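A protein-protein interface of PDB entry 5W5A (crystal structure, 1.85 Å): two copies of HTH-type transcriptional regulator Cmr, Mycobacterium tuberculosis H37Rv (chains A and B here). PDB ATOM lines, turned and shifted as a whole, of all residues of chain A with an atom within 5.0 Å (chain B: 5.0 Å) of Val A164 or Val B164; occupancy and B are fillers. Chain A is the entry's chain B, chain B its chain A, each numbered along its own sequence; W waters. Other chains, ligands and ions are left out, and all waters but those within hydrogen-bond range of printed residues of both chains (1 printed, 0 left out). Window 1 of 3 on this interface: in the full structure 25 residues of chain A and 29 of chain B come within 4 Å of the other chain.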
ATOM      1  N   CYS A  39     -22.435 -35.179   5.877  1.00  0.00           N
ATOM      2  CA  CYS A  39     -22.455 -33.968   5.028  1.00  0.00           C
ATOM      3  C   CYS A  39     -23.810 -33.748   4.358  1.00  0.00           C
ATOM      4  O   CYS A  39     -23.938 -32.899   3.471  1.00  0.00           O
ATOM      5  CB  CYS A  39     -21.379 -34.066   3.940  1.00  0.00           C
ATOM      6  SG  CYS A  39     -19.699 -34.114   4.575  1.00  0.00           S
ATOM      7  N   ILE A 114     -23.542 -32.952  -3.061  1.00  0.00           N
ATOM      8  CA  ILE A 114     -22.098 -32.870  -2.844  1.00  0.00           C
ATOM      9  C   ILE A 114     -21.338 -33.974  -3.589  1.00  0.00           C
ATOM     10  O   ILE A 114     -20.314 -33.699  -4.249  1.00  0.00           O
ATOM     11  CB  ILE A 114     -21.772 -32.850  -1.327  1.00  0.00           C
ATOM     12  CG1 ILE A 114     -22.274 -31.517  -0.744  1.00  0.00           C
ATOM     13  CG2 ILE A 114     -20.271 -32.955  -1.096  1.00  0.00           C
ATOM     14  CD1 ILE A 114     -22.087 -31.326   0.756  1.00  0.00           C
ATOM     15  N   SER A 159     -24.587 -23.467   1.861  1.00  0.00           N
ATOM     16  CA  SER A 159     -24.968 -24.808   2.339  1.00  0.00           C
ATOM     17  C   SER A 159     -23.808 -25.780   2.272  1.00  0.00           C
ATOM     18  O   SER A 159     -23.518 -26.471   3.249  1.00  0.00           O
ATOM     19  CB  SER A 159     -26.140 -25.353   1.525  1.00  0.00           C
ATOM     20  OG  SER A 159     -26.382 -26.735   1.854  1.00  0.00           O
ATOM     21  N   VAL A 160     -23.129 -25.848   1.123  1.00  0.00           N
ATOM     22  CA  VAL A 160     -22.021 -26.790   0.962  1.00  0.00           C
ATOM     23  C   VAL A 160     -20.896 -26.483   1.940  1.00  0.00           C
ATOM     24  O   VAL A 160     -20.361 -27.397   2.568  1.00  0.00           O
ATOM     25  CB  VAL A 160     -21.480 -26.776  -0.488  1.00  0.00           C
ATOM     26  CG1 VAL A 160     -20.134 -27.508  -0.562  1.00  0.00           C
ATOM     27  CG2 VAL A 160     -22.495 -27.395  -1.409  1.00  0.00           C
ATOM     28  N   ALA A 161     -20.528 -25.196   2.071  1.00  0.00           N
ATOM     29  CA  ALA A 161     -19.494 -24.770   3.019  1.00  0.00           C
ATOM     30  C   ALA A 161     -19.846 -25.200   4.436  1.00  0.00           C
ATOM     31  O   ALA A 161     -19.014 -25.745   5.178  1.00  0.00           O
ATOM     32  CB  ALA A 161     -19.297 -23.237   2.974  1.00  0.00           C
ATOM     33  N   GLN A 162     -21.079 -24.931   4.833  1.00  0.00           N
ATOM     34  CA  GLN A 162     -21.521 -25.353   6.165  1.00  0.00           C
ATOM     35  C   GLN A 162     -21.444 -26.868   6.372  1.00  0.00           C
ATOM     36  O   GLN A 162     -20.932 -27.349   7.390  1.00  0.00           O
ATOM     37  CB  GLN A 162     -22.946 -24.879   6.380  1.00  0.00           C
ATOM     38  CG  GLN A 162     -23.536 -25.200   7.728  1.00  0.00           C
ATOM     39  CD  GLN A 162     -24.875 -24.495   7.893  1.00  0.00           C
ATOM     40  OE1 GLN A 162     -25.166 -23.529   7.172  1.00  0.00           O
ATOM     41  NE2 GLN A 162     -25.700 -24.978   8.819  1.00  0.00           N
ATOM     42  N   ARG A 163     -21.937 -27.624   5.405  1.00  0.00           N
ATOM     43  CA  ARG A 163     -22.076 -29.055   5.629  1.00  0.00           C
ATOM     44  C   ARG A 163     -20.712 -29.747   5.671  1.00  0.00           C
ATOM     45  O   ARG A 163     -20.472 -30.587   6.536  1.00  0.00           O
ATOM     46  CB  ARG A 163     -22.984 -29.666   4.554  1.00  0.00           C
ATOM     47  CG  ARG A 163     -24.469 -29.269   4.767  1.00  0.00           C
ATOM     48  CD  ARG A 163     -25.156 -29.152   3.426  1.00  0.00           C
ATOM     49  NE  ARG A 163     -25.158 -30.456   2.753  1.00  0.00           N
ATOM     50  CZ  ARG A 163     -25.600 -30.671   1.520  1.00  0.00           C
ATOM     51  NH1 ARG A 163     -26.074 -29.651   0.768  1.00  0.00           N
ATOM     52  NH2 ARG A 163     -25.539 -31.897   1.033  1.00  0.00           N
ATOM     53  N   VAL A 164     -19.808 -29.386   4.763  1.00  0.00           N
ATOM     54  CA  VAL A 164     -18.514 -30.084   4.770  1.00  0.00           C
ATOM     55  C   VAL A 164     -17.652 -29.625   5.943  1.00  0.00           C
ATOM     56  O   VAL A 164     -16.886 -30.417   6.502  1.00  0.00           O
ATOM     57  CB  VAL A 164     -17.754 -29.901   3.416  1.00  0.00           C
ATOM     58  CG1 VAL A 164     -18.563 -30.472   2.281  1.00  0.00           C
ATOM     59  CG2 VAL A 164     -17.462 -28.413   3.111  1.00  0.00           C
ATOM     60  N   SER A 165     -17.774 -28.361   6.338  1.00  0.00           N
ATOM     61  CA  SER A 165     -16.941 -27.858   7.426  1.00  0.00           C
ATOM     62  C   SER A 165     -17.365 -28.475   8.738  1.00  0.00           C
ATOM     63  O   SER A 165     -16.535 -28.776   9.591  1.00  0.00           O
ATOM     64  CB  SER A 165     -17.013 -26.326   7.531  1.00  0.00           C
ATOM     65  OG  SER A 165     -16.550 -25.709   6.344  1.00  0.00           O
ATOM     66  N   THR A 166     -18.671 -28.656   8.900  1.00  0.00           N
ATOM     67  CA  THR A 166     -19.197 -29.275  10.118  1.00  0.00           C
ATOM     68  C   THR A 166     -18.640 -30.687  10.299  1.00  0.00           C
ATOM     69  O   THR A 166     -18.190 -31.044  11.379  1.00  0.00           O
ATOM     70  CB  THR A 166     -20.746 -29.294  10.104  1.00  0.00           C
ATOM     71  OG1 THR A 166     -21.193 -27.946  10.172  1.00  0.00           O
ATOM     72  CG2 THR A 166     -21.291 -30.055  11.306  1.00  0.00           C
ATOM     73  N   ALA A 167     -18.660 -31.481   9.245  1.00  0.00           N
ATOM     74  CA  ALA A 167     -18.054 -32.799   9.306  1.00  0.00           C
ATOM     75  C   ALA A 167     -16.552 -32.744   9.645  1.00  0.00           C
ATOM     76  O   ALA A 167     -16.045 -33.541  10.450  1.00  0.00           O
ATOM     77  CB  ALA A 167     -18.266 -33.520   7.987  1.00  0.00           C
ATOM     78  N   GLN A 168     -15.830 -31.826   9.003  1.00  0.00           N
ATOM     79  CA  GLN A 168     -14.399 -31.750   9.203  1.00  0.00           C
ATOM     80  C   GLN A 168     -14.092 -31.418  10.640  1.00  0.00           C
ATOM     81  O   GLN A 168     -13.176 -31.971  11.264  1.00  0.00           O
ATOM     82  CB  GLN A 168     -13.784 -30.674   8.271  1.00  0.00           C
ATOM     83  CG  GLN A 168     -12.253 -30.636   8.416  1.00  0.00           C
ATOM     84  CD  GLN A 168     -11.637 -29.333   7.953  1.00  0.00           C
ATOM     85  OE1 GLN A 168     -12.335 -28.451   7.468  1.00  0.00           O
ATOM     86  NE2 GLN A 168     -10.318 -29.206   8.108  1.00  0.00           N
ATOM     87  N   CYS B  39      -7.187 -26.536   3.905  1.00  0.00           N
ATOM     88  CA  CYS B  39      -8.322 -26.295   2.990  1.00  0.00           C
ATOM     89  C   CYS B  39      -8.050 -25.085   2.075  1.00  0.00           C
ATOM     90  O   CYS B  39      -8.955 -24.566   1.418  1.00  0.00           O
ATOM     91  CB  CYS B  39      -9.625 -26.062   3.769  1.00  0.00           C
ATOM     92  SG  CYS B  39     -10.117 -27.442   4.848  1.00  0.00           S
ATOM     93  N   ILE B 114     -13.627 -19.530   2.841  1.00  0.00           N
ATOM     94  CA  ILE B 114     -14.491 -20.418   3.588  1.00  0.00           C
ATOM     95  C   ILE B 114     -14.933 -19.793   4.931  1.00  0.00           C
ATOM     96  O   ILE B 114     -16.121 -19.805   5.221  1.00  0.00           O
ATOM     97  CB  ILE B 114     -13.837 -21.812   3.798  1.00  0.00           C
ATOM     98  CG1 ILE B 114     -13.631 -22.466   2.420  1.00  0.00           C
ATOM     99  CG2 ILE B 114     -14.724 -22.739   4.722  1.00  0.00           C
ATOM    100  CD1 ILE B 114     -12.801 -23.759   2.447  1.00  0.00           C
ATOM    101  N   SER B 159     -15.088 -25.892  -5.798  1.00  0.00           N
ATOM    102  CA  SER B 159     -13.813 -25.651  -5.113  1.00  0.00           C
ATOM    103  C   SER B 159     -13.922 -25.878  -3.588  1.00  0.00           C
ATOM    104  O   SER B 159     -13.148 -26.628  -2.995  1.00  0.00           O
ATOM    105  CB  SER B 159     -13.320 -24.224  -5.432  1.00  0.00           C
ATOM    106  OG  SER B 159     -12.295 -23.810  -4.549  1.00  0.00           O
ATOM    107  N   VAL B 160     -14.909 -25.279  -2.953  1.00  0.00           N
ATOM    108  CA  VAL B 160     -15.112 -25.482  -1.526  1.00  0.00           C
ATOM    109  C   VAL B 160     -15.364 -26.972  -1.201  1.00  0.00           C
ATOM    110  O   VAL B 160     -14.767 -27.524  -0.274  1.00  0.00           O
ATOM    111  CB  VAL B 160     -16.297 -24.631  -1.005  1.00  0.00           C
ATOM    112  CG1 VAL B 160     -16.631 -25.006   0.429  1.00  0.00           C
ATOM    113  CG2 VAL B 160     -15.922 -23.107  -1.031  1.00  0.00           C
ATOM    114  N   ALA B 161     -16.211 -27.614  -1.987  1.00  0.00           N
ATOM    115  CA  ALA B 161     -16.499 -29.031  -1.767  1.00  0.00           C
ATOM    116  C   ALA B 161     -15.197 -29.840  -1.835  1.00  0.00           C
ATOM    117  O   ALA B 161     -14.887 -30.656  -0.949  1.00  0.00           O
ATOM    118  CB  ALA B 161     -17.501 -29.527  -2.789  1.00  0.00           C
ATOM    119  N   GLN B 162     -14.419 -29.603  -2.875  1.00  0.00           N
ATOM    120  CA  GLN B 162     -13.180 -30.374  -3.087  1.00  0.00           C
ATOM    121  C   GLN B 162     -12.146 -30.116  -1.998  1.00  0.00           C
ATOM    122  O   GLN B 162     -11.504 -31.054  -1.477  1.00  0.00           O
ATOM    123  CB  GLN B 162     -12.593 -30.052  -4.478  1.00  0.00           C
ATOM    124  CG  GLN B 162     -11.564 -31.066  -4.951  1.00  0.00           C
ATOM    125  CD  GLN B 162     -12.131 -32.498  -5.165  1.00  0.00           C
ATOM    126  OE1 GLN B 162     -12.889 -32.757  -6.111  1.00  0.00           O
ATOM    127  NE2 GLN B 162     -11.741 -33.424  -4.292  1.00  0.00           N
ATOM    128  N   ARG B 163     -11.949 -28.852  -1.652  1.00  0.00           N
ATOM    129  CA  ARG B 163     -10.929 -28.502  -0.658  1.00  0.00           C
ATOM    130  C   ARG B 163     -11.221 -29.112   0.702  1.00  0.00           C
ATOM    131  O   ARG B 163     -10.354 -29.756   1.308  1.00  0.00           O
ATOM    132  CB  ARG B 163     -10.817 -26.994  -0.529  1.00  0.00           C
ATOM    133  CG  ARG B 163     -10.085 -26.402  -1.746  1.00  0.00           C
ATOM    134  CD  ARG B 163     -10.608 -24.975  -2.057  1.00  0.00           C
ATOM    135  NE  ARG B 163     -10.292 -24.057  -0.969  1.00  0.00           N
ATOM    136  CZ  ARG B 163     -10.758 -22.818  -0.870  1.00  0.00           C
ATOM    137  NH1 ARG B 163     -11.639 -22.352  -1.760  1.00  0.00           N
ATOM    138  NH2 ARG B 163     -10.364 -22.057   0.138  1.00  0.00           N
ATOM    139  N   VAL B 164     -12.447 -28.954   1.172  1.00  0.00           N
ATOM    140  CA  VAL B 164     -12.755 -29.509   2.484  1.00  0.00           C
ATOM    141  C   VAL B 164     -12.871 -31.034   2.495  1.00  0.00           C
ATOM    142  O   VAL B 164     -12.446 -31.676   3.482  1.00  0.00           O
ATOM    143  CB  VAL B 164     -14.028 -28.862   3.056  1.00  0.00           C
ATOM    144  CG1 VAL B 164     -14.269 -29.356   4.480  1.00  0.00           C
ATOM    145  CG2 VAL B 164     -13.864 -27.342   3.054  1.00  0.00           C
ATOM    146  N   SER B 165     -13.429 -31.626   1.436  1.00  0.00           N
ATOM    147  CA  SER B 165     -13.536 -33.088   1.386  1.00  0.00           C
ATOM    148  C   SER B 165     -12.167 -33.741   1.342  1.00  0.00           C
ATOM    149  O   SER B 165     -11.956 -34.806   1.933  1.00  0.00           O
ATOM    150  CB  SER B 165     -14.357 -33.559   0.182  1.00  0.00           C
ATOM    151  OG  SER B 165     -13.716 -33.225  -1.031  1.00  0.00           O
ATOM    152  N   THR B 166     -11.238 -33.112   0.633  1.00  0.00           N
ATOM    153  CA  THR B 166      -9.885 -33.649   0.562  1.00  0.00           C
ATOM    154  C   THR B 166      -9.280 -33.734   1.971  1.00  0.00           C
ATOM    155  O   THR B 166      -8.675 -34.746   2.337  1.00  0.00           O
ATOM    156  CB  THR B 166      -9.015 -32.803  -0.376  1.00  0.00           C
ATOM    157  OG1 THR B 166      -9.427 -33.077  -1.712  1.00  0.00           O
ATOM    158  CG2 THR B 166      -7.557 -33.150  -0.238  1.00  0.00           C
ATOM    159  N   ALA B 167      -9.489 -32.707   2.785  1.00  0.00           N
ATOM    160  CA  ALA B 167      -9.034 -32.749   4.183  1.00  0.00           C
ATOM    161  C   ALA B 167      -9.802 -33.781   5.015  1.00  0.00           C
ATOM    162  O   ALA B 167      -9.206 -34.518   5.825  1.00  0.00           O
ATOM    163  CB  ALA B 167      -9.159 -31.380   4.835  1.00  0.00           C
ATOM    164  N   GLN B 168     -11.110 -33.842   4.795  1.00  0.00           N
ATOM    165  CA  GLN B 168     -11.961 -34.828   5.460  1.00  0.00           C
ATOM    166  C   GLN B 168     -11.459 -36.263   5.204  1.00  0.00           C
ATOM    167  O   GLN B 168     -11.428 -37.140   6.123  1.00  0.00           O
ATOM    168  CB  GLN B 168     -13.417 -34.670   4.973  1.00  0.00           C
ATOM    169  CG  GLN B 168     -14.385 -35.547   5.752  1.00  0.00           C
ATOM    170  CD  GLN B 168     -15.765 -35.620   5.132  1.00  0.00           C
ATOM    171  OE1 GLN B 168     -16.013 -35.080   4.047  1.00  0.00           O
ATOM    172  NE2 GLN B 168     -16.673 -36.293   5.816  1.00  0.00           N
HETATM  173  O   HOH W   1     -17.724 -34.817   1.580  1.00  0.00           O
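SG of Cys B39 is in hydrogen-bond range of OE1 of Gln A168 (3.6 Å).
O of Cys B39 is in hydrogen-bond range of NE of Arg B163 (2.8 Å).
The backbone carbonyl oxygen of Ala B161 is in hydrogen-bond range of the side-chain hydroxyl of Ser B165 (2.8 Å).
The guanidinium group (NE) of Arg A163 lies within hydrogen-bond range of the backbone carbonyl oxygen (O) of Cys A39 (2.8 Å).
The side-chain hydroxyl of Ser A165 lies within hydrogen-bond range of the backbone carbonyl oxygen of Ala A161 (2.7 Å).
Among the printed residues, pairs that only touch across the chains: Val A164 with Val B164 (3.5 Å), Gln A168 with Val B164 (3.7 Å), Ser A165 with Ile B114 (3.8 Å), Cys A39 with Gln B168 (3.8 Å), Ala A167 with Gln B168 (3.9 Å), Ala A161 with Val B160 (3.9 Å) and Val A160 with Ala B161 (3.996 Å).
Of the printed residues of chain B, Ala A161 touches Val B160.
Thr A166 touches none of the printed residues of chain B.
Printed residues of chain B within 4 Å of Gln A168: Cys B39 and Val B164.
Of the printed residues of chain A, Ala B161 touches Val A160 (3.996 Å).
Printed residues of chain A within 4 Å of Val B164: Val A164 and Gln A168.
Of the printed residues of chain A, Gln B168 touches Cys A39 and Ala A167.
The nearest printed residue of chain B that does not touch Val A164 is Val B160 (4.4 Å).
The nearest printed residue of chain A that does not touch Gln B168 is Gln A168 (5.0 Å).
Of the 12 printed residues of chain A, 7 touch a printed residue of chain B.
Printed residues of chain A that touch a printed residue of chain B: Cys A39, Val A160, Ala A161, Val A164, Ser A165, Ala A167 and Gln A168.
Hydrophobic or aromatic side chains of chain A that line the printed part of chain B: Val A160, Val A164 and Ala A167.
Of the 12 printed residues of chain B, 6 touch a printed residue of chain A.
Hydrophobic or aromatic side chains of chain B that line the printed part of chain A: Ile B114, Val B160, Ala B161 and Val B164.
Among the printed residues, 8 pairs touch across the chains.
Among the printed residues, no Asp or Glu carboxylate lies within 4 Å of a Lys or Arg side-chain nitrogen of the other chain.
Val B164 touches its own counterpart, Val A164.
Ser A165 touches Ile B114, but with the chains exchanged Ile A114 does not touch Ser B165 (6.1 Å).
Ala A167 touches Gln B168, but with the chains exchanged Gln A168 does not touch Ala B167 (4.1 Å).
Gln A168 touches Val B164, but with the chains exchanged Val A164 does not touch Gln B168 (5.3 Å).
Of the 8 pairs that touch across the chains among the printed residues, 5 have their exchanged pair printed and touching as well.
Water W1 bridges OE1 of Gln B168 (3.0 Å) and SG of Cys A39 (3.7 Å).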
